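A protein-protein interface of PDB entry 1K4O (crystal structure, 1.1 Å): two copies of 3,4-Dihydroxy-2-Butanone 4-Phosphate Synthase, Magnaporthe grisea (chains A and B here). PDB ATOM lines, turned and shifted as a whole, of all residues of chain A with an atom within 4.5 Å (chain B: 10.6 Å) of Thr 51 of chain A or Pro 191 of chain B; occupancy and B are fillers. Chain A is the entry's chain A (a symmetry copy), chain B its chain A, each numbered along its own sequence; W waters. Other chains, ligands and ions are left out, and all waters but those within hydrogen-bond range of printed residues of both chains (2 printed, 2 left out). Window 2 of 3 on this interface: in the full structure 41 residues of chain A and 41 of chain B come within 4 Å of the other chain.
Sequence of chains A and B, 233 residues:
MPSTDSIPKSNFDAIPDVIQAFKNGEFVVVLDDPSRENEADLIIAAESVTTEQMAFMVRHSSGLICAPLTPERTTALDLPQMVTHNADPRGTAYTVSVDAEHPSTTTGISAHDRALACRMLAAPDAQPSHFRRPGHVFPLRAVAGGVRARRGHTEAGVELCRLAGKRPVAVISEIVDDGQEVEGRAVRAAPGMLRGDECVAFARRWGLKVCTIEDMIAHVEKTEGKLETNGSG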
ATOM      1  N   VAL A  49      20.590   6.878   4.658  1.00  0.00           N
ATOM      2  CA  VAL A  49      20.896   5.549   4.154  1.00  0.00           C
ATOM      3  C   VAL A  49      21.489   4.709   5.254  1.00  0.00           C
ATOM      4  O   VAL A  49      22.429   5.143   5.936  1.00  0.00           O
ATOM      5  CB  VAL A  49      21.731   5.591   2.880  1.00  0.00           C
ATOM      6  CG1 VAL A  49      23.096   6.270   3.070  1.00  0.00           C
ATOM      7  CG2 VAL A  49      21.904   4.191   2.295  1.00  0.00           C
ATOM      8  N   THR A  50      20.938   3.512   5.458  1.00  0.00           N
ATOM      9  CA  THR A  50      21.410   2.711   6.598  1.00  0.00           C
ATOM     10  C   THR A  50      22.534   1.753   6.252  1.00  0.00           C
ATOM     11  O   THR A  50      22.803   1.509   5.062  1.00  0.00           O
ATOM     12  CB  THR A  50      20.265   1.911   7.243  1.00  0.00           C
ATOM     13  OG1 THR A  50      19.978   0.787   6.398  1.00  0.00           O
ATOM     14  CG2 THR A  50      19.004   2.801   7.398  1.00  0.00           C
ATOM     15  N   THR A  51      23.202   1.219   7.247  1.00  0.00           N
ATOM     16  CA  THR A  51      24.252   0.257   6.980  1.00  0.00           C
ATOM     17  C   THR A  51      23.715  -0.915   6.203  1.00  0.00           C
ATOM     18  O   THR A  51      24.334  -1.389   5.230  1.00  0.00           O
ATOM     19  CB  THR A  51      24.834  -0.239   8.300  1.00  0.00           C
ATOM     20  OG1 THR A  51      25.498   0.844   8.929  1.00  0.00           O
ATOM     21  CG2 THR A  51      25.825  -1.373   8.085  1.00  0.00           C
ATOM     22  N   GLU A  52      22.533  -1.424   6.611  1.00  0.00           N
ATOM     23  CA  GLU A  52      21.913  -2.570   5.979  1.00  0.00           C
ATOM     24  C   GLU A  52      21.454  -2.260   4.560  1.00  0.00           C
ATOM     25  O   GLU A  52      21.512  -3.124   3.660  1.00  0.00           O
ATOM     26  CB  GLU A  52      20.760  -3.132   6.855  1.00  0.00           C
ATOM     27  CG  GLU A  52      21.264  -3.646   8.208  1.00  0.00           C
ATOM     28  CD  GLU A  52      21.620  -2.591   9.247  1.00  0.00           C
ATOM     29  OE1 GLU A  52      22.438  -2.844  10.120  1.00  0.00           O
ATOM     30  OE2 GLU A  52      21.041  -1.429   9.148  1.00  0.00           O
ATOM     31  N   GLN A  53      20.973  -1.041   4.341  1.00  0.00           N
ATOM     32  CA  GLN A  53      20.597  -0.689   2.979  1.00  0.00           C
ATOM     33  C   GLN A  53      21.848  -0.643   2.100  1.00  0.00           C
ATOM     34  O   GLN A  53      21.823  -1.068   0.945  1.00  0.00           O
ATOM     35  CB  GLN A  53      19.923   0.697   2.924  1.00  0.00           C
ATOM     36  CG  GLN A  53      18.471   0.667   3.488  1.00  0.00           C
ATOM     37  CD  GLN A  53      17.834   2.027   3.400  1.00  0.00           C
ATOM     38  OE1 GLN A  53      18.391   3.047   3.868  1.00  0.00           O
ATOM     39  NE2 GLN A  53      16.623   2.024   2.846  1.00  0.00           N
ATOM     40  N   MET A  54      22.925  -0.067   2.632  1.00  0.00           N
ATOM     41  CA  MET A  54      24.153   0.040   1.843  1.00  0.00           C
ATOM     42  C   MET A  54      24.671  -1.347   1.487  1.00  0.00           C
ATOM     43  O   MET A  54      25.169  -1.586   0.373  1.00  0.00           O
ATOM     44  CB  MET A  54      25.198   0.854   2.620  1.00  0.00           C
ATOM     45  CG  MET A  54      26.508   1.048   1.817  1.00  0.00           C
ATOM     46  SD  MET A  54      26.301   1.935   0.234  1.00  0.00           S
ATOM     47  CE  MET A  54      25.928   3.605   0.862  1.00  0.00           C
ATOM     48  N   ALA A  55      24.556  -2.289   2.424  1.00  0.00           N
ATOM     49  CA  ALA A  55      24.999  -3.661   2.161  1.00  0.00           C
ATOM     50  C   ALA A  55      24.209  -4.258   1.003  1.00  0.00           C
ATOM     51  O   ALA A  55      24.764  -4.943   0.112  1.00  0.00           O
ATOM     52  CB  ALA A  55      24.937  -4.524   3.417  1.00  0.00           C
ATOM     53  N   ALA A 111      30.135  -1.512   4.327  1.00  0.00           N
ATOM     54  CA  ALA A 111      28.784  -0.929   4.189  1.00  0.00           C
ATOM     55  C   ALA A 111      28.566   0.131   5.257  1.00  0.00           C
ATOM     56  O   ALA A 111      27.971   1.187   4.991  1.00  0.00           O
ATOM     57  CB  ALA A 111      27.676  -1.983   4.276  1.00  0.00           C
ATOM     58  N   HIS A 112      29.016  -0.139   6.497  1.00  0.00           N
ATOM     59  CA  HIS A 112      28.840   0.855   7.555  1.00  0.00           C
ATOM     60  C   HIS A 112      29.520   2.163   7.185  1.00  0.00           C
ATOM     61  O   HIS A 112      28.967   3.257   7.315  1.00  0.00           O
ATOM     62  CB  HIS A 112      29.405   0.302   8.882  1.00  0.00           C
ATOM     63  CG  HIS A 112      29.644   1.332   9.922  1.00  0.00           C
ATOM     64  ND1 HIS A 112      30.771   2.153   9.956  1.00  0.00           N
ATOM     65  CD2 HIS A 112      28.827   1.699  10.968  1.00  0.00           C
ATOM     66  CE1 HIS A 112      30.638   2.950  11.021  1.00  0.00           C
ATOM     67  NE2 HIS A 112      29.477   2.706  11.638  1.00  0.00           N
ATOM     68  N   ALA A 115      28.000   3.997   4.034  1.00  0.00           N
ATOM     69  CA  ALA A 115      26.703   4.625   4.397  1.00  0.00           C
ATOM     70  C   ALA A 115      26.957   5.900   5.243  1.00  0.00           C
ATOM     71  O   ALA A 115      26.316   6.942   5.037  1.00  0.00           O
ATOM     72  CB  ALA A 115      25.824   3.645   5.163  1.00  0.00           C
ATOM     73  N   ILE B 175      37.288  -8.326   0.198  1.00  0.00           N
ATOM     74  CA  ILE B 175      36.238  -9.332   0.334  1.00  0.00           C
ATOM     75  C   ILE B 175      35.320  -8.887   1.461  1.00  0.00           C
ATOM     76  O   ILE B 175      35.695  -8.869   2.622  1.00  0.00           O
ATOM     77  CB  ILE B 175      36.806 -10.751   0.558  1.00  0.00           C
ATOM     78  CG1 ILE B 175      37.755 -11.134  -0.598  1.00  0.00           C
ATOM     79  CG2 ILE B 175      35.634 -11.734   0.552  1.00  0.00           C
ATOM     80  CD1 ILE B 175      38.542 -12.411  -0.303  1.00  0.00           C
ATOM     81  N   VAL B 176      34.084  -8.512   1.114  1.00  0.00           N
ATOM     82  CA  VAL B 176      33.140  -8.057   2.136  1.00  0.00           C
ATOM     83  C   VAL B 176      32.307  -9.219   2.670  1.00  0.00           C
ATOM     84  O   VAL B 176      32.295 -10.327   2.155  1.00  0.00           O
ATOM     85  CB  VAL B 176      32.176  -7.006   1.543  1.00  0.00           C
ATOM     86  CG1 VAL B 176      32.951  -5.824   0.949  1.00  0.00           C
ATOM     87  CG2 VAL B 176      31.272  -7.650   0.487  1.00  0.00           C
ATOM     88  N   ASP B 177      31.608  -8.966   3.792  1.00  0.00           N
ATOM     89  CA  ASP B 177      30.651  -9.888   4.324  1.00  0.00           C
ATOM     90  C   ASP B 177      29.323  -9.217   3.929  1.00  0.00           C
ATOM     91  O   ASP B 177      28.964  -8.157   4.463  1.00  0.00           O
ATOM     92  CB  ASP B 177      30.763 -10.081   5.841  1.00  0.00           C
ATOM     93  CG  ASP B 177      29.707 -11.045   6.349  1.00  0.00           C
ATOM     94  OD1 ASP B 177      28.755 -11.440   5.704  1.00  0.00           O
ATOM     95  OD2 ASP B 177      29.938 -11.369   7.574  1.00  0.00           O
ATOM     96  N   ASP B 178      28.655  -9.793   2.945  1.00  0.00           N
ATOM     97  CA  ASP B 178      27.415  -9.174   2.519  1.00  0.00           C
ATOM     98  C   ASP B 178      26.233  -9.406   3.471  1.00  0.00           C
ATOM     99  O   ASP B 178      25.102  -8.982   3.159  1.00  0.00           O
ATOM    100  CB  ASP B 178      27.023  -9.567   1.097  1.00  0.00           C
ATOM    101  CG  ASP B 178      26.946 -11.047   1.028  1.00  0.00           C
ATOM    102  OD1 ASP B 178      26.827 -11.730   2.036  1.00  0.00           O
ATOM    103  OD2 ASP B 178      27.061 -11.514  -0.187  1.00  0.00           O
ATOM    104  N   GLY B 179      26.468 -10.043   4.619  1.00  0.00           N
ATOM    105  CA  GLY B 179      25.369 -10.264   5.526  1.00  0.00           C
ATOM    106  C   GLY B 179      24.352 -11.252   4.934  1.00  0.00           C
ATOM    107  O   GLY B 179      24.596 -12.053   4.007  1.00  0.00           O
ATOM    108  N   GLN B 180      23.147 -11.171   5.487  1.00  0.00           N
ATOM    109  CA  GLN B 180      22.109 -12.080   5.046  1.00  0.00           C
ATOM    110  C   GLN B 180      21.013 -11.402   4.277  1.00  0.00           C
ATOM    111  O   GLN B 180      20.588 -10.288   4.615  1.00  0.00           O
ATOM    112  CB  GLN B 180      21.447 -12.803   6.236  1.00  0.00           C
ATOM    113  CG  GLN B 180      22.347 -13.957   6.735  1.00  0.00           C
ATOM    114  CD  GLN B 180      23.376 -13.427   7.708  1.00  0.00           C
ATOM    115  OE1 GLN B 180      24.568 -13.738   7.596  1.00  0.00           O
ATOM    116  NE2 GLN B 180      22.920 -12.563   8.621  1.00  0.00           N
ATOM    117  N   GLU B 181      20.559 -12.138   3.283  1.00  0.00           N
ATOM    118  CA  GLU B 181      19.424 -11.692   2.484  1.00  0.00           C
ATOM    119  C   GLU B 181      18.200 -11.615   3.398  1.00  0.00           C
ATOM    120  O   GLU B 181      18.117 -12.350   4.368  1.00  0.00           O
ATOM    121  CB  GLU B 181      19.081 -12.729   1.382  1.00  0.00           C
ATOM    122  CG  GLU B 181      17.700 -12.455   0.760  1.00  0.00           C
ATOM    123  CD  GLU B 181      17.381 -13.344  -0.413  1.00  0.00           C
ATOM    124  OE1 GLU B 181      18.062 -14.309  -0.672  1.00  0.00           O
ATOM    125  OE2 GLU B 181      16.331 -12.995  -1.131  1.00  0.00           O
ATOM    126  N   VAL B 182      17.290 -10.713   3.078  1.00  0.00           N
ATOM    127  CA  VAL B 182      16.035 -10.546   3.835  1.00  0.00           C
ATOM    128  C   VAL B 182      14.988 -10.589   2.747  1.00  0.00           C
ATOM    129  O   VAL B 182      14.950  -9.703   1.883  1.00  0.00           O
ATOM    130  CB  VAL B 182      16.012  -9.227   4.631  1.00  0.00           C
ATOM    131  CG1 VAL B 182      14.625  -9.062   5.314  1.00  0.00           C
ATOM    132  CG2 VAL B 182      17.177  -9.183   5.656  1.00  0.00           C
ATOM    133  N   ALA B 186      14.890  -4.554   0.692  1.00  0.00           N
ATOM    134  CA  ALA B 186      16.154  -4.051   0.153  1.00  0.00           C
ATOM    135  C   ALA B 186      17.135  -3.699   1.243  1.00  0.00           C
ATOM    136  O   ALA B 186      17.575  -2.559   1.336  1.00  0.00           O
ATOM    137  CB  ALA B 186      15.891  -2.863  -0.799  1.00  0.00           C
ATOM    138  N   VAL B 187      17.499  -4.710   2.032  1.00  0.00           N
ATOM    139  CA  VAL B 187      18.452  -4.582   3.119  1.00  0.00           C
ATOM    140  C   VAL B 187      19.174  -5.906   3.242  1.00  0.00           C
ATOM    141  O   VAL B 187      18.660  -6.941   2.779  1.00  0.00           O
ATOM    142  CB  VAL B 187      17.820  -4.296   4.500  1.00  0.00           C
ATOM    143  CG1 VAL B 187      17.194  -2.897   4.570  1.00  0.00           C
ATOM    144  CG2 VAL B 187      16.750  -5.338   4.845  1.00  0.00           C
ATOM    145  N   ARG B 188      20.353  -5.914   3.854  1.00  0.00           N
ATOM    146  CA  ARG B 188      21.041  -7.159   4.184  1.00  0.00           C
ATOM    147  C   ARG B 188      21.368  -7.047   5.651  1.00  0.00           C
ATOM    148  O   ARG B 188      21.918  -6.044   6.115  1.00  0.00           O
ATOM    149  CB  ARG B 188      22.354  -7.435   3.456  1.00  0.00           C
ATOM    150  CG  ARG B 188      22.296  -7.255   1.964  1.00  0.00           C
ATOM    151  CD  ARG B 188      22.012  -8.514   1.214  1.00  0.00           C
ATOM    152  NE  ARG B 188      22.958  -9.587   1.498  1.00  0.00           N
ATOM    153  CZ  ARG B 188      22.839 -10.758   0.882  1.00  0.00           C
ATOM    154  NH1 ARG B 188      21.881 -10.918  -0.045  1.00  0.00           N
ATOM    155  NH2 ARG B 188      23.681 -11.769   1.191  1.00  0.00           N
ATOM    156  N   ALA B 189      21.051  -8.080   6.408  1.00  0.00           N
ATOM    157  CA  ALA B 189      21.321  -8.016   7.835  1.00  0.00           C
ATOM    158  C   ALA B 189      22.744  -8.410   8.200  1.00  0.00           C
ATOM    159  O   ALA B 189      23.356  -9.288   7.563  1.00  0.00           O
ATOM    160  CB  ALA B 189      20.376  -8.993   8.505  1.00  0.00           C
ATOM    161  N   ALA B 190      23.243  -7.730   9.238  1.00  0.00           N
ATOM    162  CA  ALA B 190      24.551  -8.014   9.786  1.00  0.00           C
ATOM    163  C   ALA B 190      25.685  -8.092   8.761  1.00  0.00           C
ATOM    164  O   ALA B 190      26.483  -9.034   8.781  1.00  0.00           O
ATOM    165  CB  ALA B 190      24.458  -9.349  10.536  1.00  0.00           C
ATOM    166  N   PRO B 191      25.831  -7.097   7.900  1.00  0.00           N
ATOM    167  CA  PRO B 191      26.953  -7.101   6.937  1.00  0.00           C
ATOM    168  C   PRO B 191      28.266  -6.682   7.666  1.00  0.00           C
ATOM    169  O   PRO B 191      28.273  -6.254   8.822  1.00  0.00           O
ATOM    170  CB  PRO B 191      26.574  -6.000   5.962  1.00  0.00           C
ATOM    171  CG  PRO B 191      25.831  -4.999   6.853  1.00  0.00           C
ATOM    172  CD  PRO B 191      24.988  -5.880   7.755  1.00  0.00           C
ATOM    173  N   GLY B 192      29.406  -6.801   6.971  1.00  0.00           N
ATOM    174  CA  GLY B 192      30.696  -6.427   7.555  1.00  0.00           C
ATOM    175  C   GLY B 192      31.763  -6.670   6.525  1.00  0.00           C
ATOM    176  O   GLY B 192      31.536  -6.574   5.312  1.00  0.00           O
ATOM    177  N   MET B 193      32.927  -7.011   7.037  1.00  0.00           N
ATOM    178  CA  MET B 193      34.094  -7.394   6.237  1.00  0.00           C
ATOM    179  C   MET B 193      34.416  -8.827   6.562  1.00  0.00           C
ATOM    180  O   MET B 193      34.214  -9.212   7.689  1.00  0.00           O
ATOM    181  CB  MET B 193      35.359  -6.514   6.465  1.00  0.00           C
ATOM    182  CG  MET B 193      35.087  -5.054   6.132  1.00  0.00           C
ATOM    183  SD  MET B 193      34.493  -4.781   4.450  1.00  0.00           S
ATOM    184  CE  MET B 193      36.046  -5.142   3.568  1.00  0.00           C
ATOM    185  N   LEU B 194      34.891  -9.628   5.620  1.00  0.00           N
ATOM    186  CA  LEU B 194      35.229 -10.987   5.959  1.00  0.00           C
ATOM    187  C   LEU B 194      36.539 -10.981   6.709  1.00  0.00           C
ATOM    188  O   LEU B 194      37.446 -10.288   6.282  1.00  0.00           O
ATOM    189  CB  LEU B 194      35.362 -11.835   4.673  1.00  0.00           C
ATOM    190  CG  LEU B 194      34.737 -13.218   4.767  1.00  0.00           C
ATOM    191  CD1 LEU B 194      33.291 -13.193   5.305  1.00  0.00           C
ATOM    192  CD2 LEU B 194      34.762 -13.848   3.379  1.00  0.00           C
ATOM    193  N   ARG B 195      36.694 -11.729   7.802  1.00  0.00           N
ATOM    194  CA  ARG B 195      37.955 -11.719   8.518  1.00  0.00           C
ATOM    195  C   ARG B 195      38.544 -13.108   8.797  1.00  0.00           C
ATOM    196  O   ARG B 195      37.824 -14.097   8.917  1.00  0.00           O
ATOM    197  CB  ARG B 195      37.748 -11.120   9.898  1.00  0.00           C
ATOM    198  CG  ARG B 195      36.885  -9.885   9.866  1.00  0.00           C
ATOM    199  CD  ARG B 195      37.661  -8.589   9.784  1.00  0.00           C
ATOM    200  NE  ARG B 195      36.801  -7.407   9.972  1.00  0.00           N
ATOM    201  CZ  ARG B 195      37.191  -6.199   9.572  1.00  0.00           C
ATOM    202  NH1 ARG B 195      38.383  -5.999   8.976  1.00  0.00           N
ATOM    203  NH2 ARG B 195      36.383  -5.147   9.743  1.00  0.00           N
ATOM    204  N   GLU B 198      37.279 -16.788   8.329  1.00  0.00           N
ATOM    205  CA  GLU B 198      36.238 -16.772   7.339  1.00  0.00           C
ATOM    206  C   GLU B 198      36.809 -16.584   5.939  1.00  0.00           C
ATOM    207  O   GLU B 198      36.240 -17.080   4.947  1.00  0.00           O
ATOM    208  CB  GLU B 198      35.067 -15.825   7.628  1.00  0.00           C
ATOM    209  CG  GLU B 198      35.384 -14.346   7.664  1.00  0.00           C
ATOM    210  CD  GLU B 198      34.880 -13.825   8.973  1.00  0.00           C
ATOM    211  OE1 GLU B 198      34.199 -12.819   9.054  1.00  0.00           O
ATOM    212  OE2 GLU B 198      35.205 -14.595   9.988  1.00  0.00           O
HETATM  213  O   HOH W   1      15.733  -0.519   1.894  1.00  0.00           O
HETATM  214  O   HOH W   2      22.183  -5.733  10.744  1.00  0.00           O
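N of Arg 188 of chain B sits at hydrogen-bond distance from O of Glu 52 of chain A (3.0 Å).
The backbone carbonyl oxygen (O) of Gly 179 of chain B is in hydrogen-bond range of the guanidinium group (NH2) of Arg 188 of chain B, at 3.0 Å. The side-chain hydroxyl (OG1) of Thr 50 of chain A sits close to the backbone NH (N) of Glu 52 of chain A (3.4 Å). The side-chain hydroxyl (OG1) of Thr 50 of chain A sits at hydrogen-bond distance from the backbone NH (N) of Gln 53 of chain A (2.9 Å). The guanidinium group of Arg 188 of chain B is in salt-bridge range of the side-chain carboxylate of Asp 178 of chain B, 3.3 Å away.
Among the printed residues, pairs that only touch across the chains: Ala 55 of chain A with Pro 191 of chain B (3.4 Å), Glu 52 of chain A with Val 187 of chain B (3.4 Å), Ala 55 of chain A with Arg 188 of chain B (3.7 Å), Thr 51 of chain A with Pro 191 of chain B (3.8 Å), Gln 53 of chain A with Ala 186 of chain B (3.9 Å) and Gln 53 of chain A with Val 187 of chain B (3.9 Å).
Thr 51 of chain A touches just one residue of chain B: Pro 191 (3.8 Å). Pro 191 of chain B touches two residues of chain A. No residue of chain B comes within 4 Å of Thr 50 of chain A. Of chain B, only Val 187 and Arg 188 come within 4 Å of Glu 52 of chain A. No residue of chain B comes within 4 Å of Ala 111 of chain A. No residue of chain B comes within 4 Å of His 112 of chain A. Printed residues of chain A within 4 Å of Arg 188 of chain B: Glu 52 and Ala 55. Printed residues of chain B within 4 Å of Gln 53 of chain A: Ala 186 (3.9 Å) and Val 187 (3.9 Å). Of the printed residues of chain A, Val 187 of chain B touches Glu 52 (3.4 Å) and Gln 53 (3.9 Å). Leu 194 of chain B touches none of the printed residues of chain A. The nearest residue of chain B that does not touch Thr 51 of chain A is Arg 188 of chain B (5.3 Å). The nearest printed residue of chain A that does not touch Pro 191 of chain B is Glu 52 of chain A (4.4 Å).
Of the 10 printed residues of chain A, 4 touch a printed residue of chain B. Printed residues of chain B that touch a printed residue of chain A: Ala 186, Val 187, Arg 188 and Pro 191. Hydrophobic or aromatic side chains of chain B that line the printed part of chain A: Val 187 and Pro 191. Among the printed residues, 7 pairs touch across the chains. Among the printed residues, no Asp or Glu carboxylate lies within 4 Å of a Lys or Arg side-chain nitrogen of the other chain.
No position is printed for both chains. Of the 7 pairs that touch across the chains among the printed residues, none has its exchanged pair printed and touching as well.
Water W2 bridges the backbone NH (N) of Ala 190 of chain B (2.7 Å) and the side-chain carboxylate (OE1) of Glu 52 of chain A (3.0 Å). Water W1 lies within hydrogen-bond range of O of Ala 186 of chain B and NE2 of Gln 53 of chain A.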
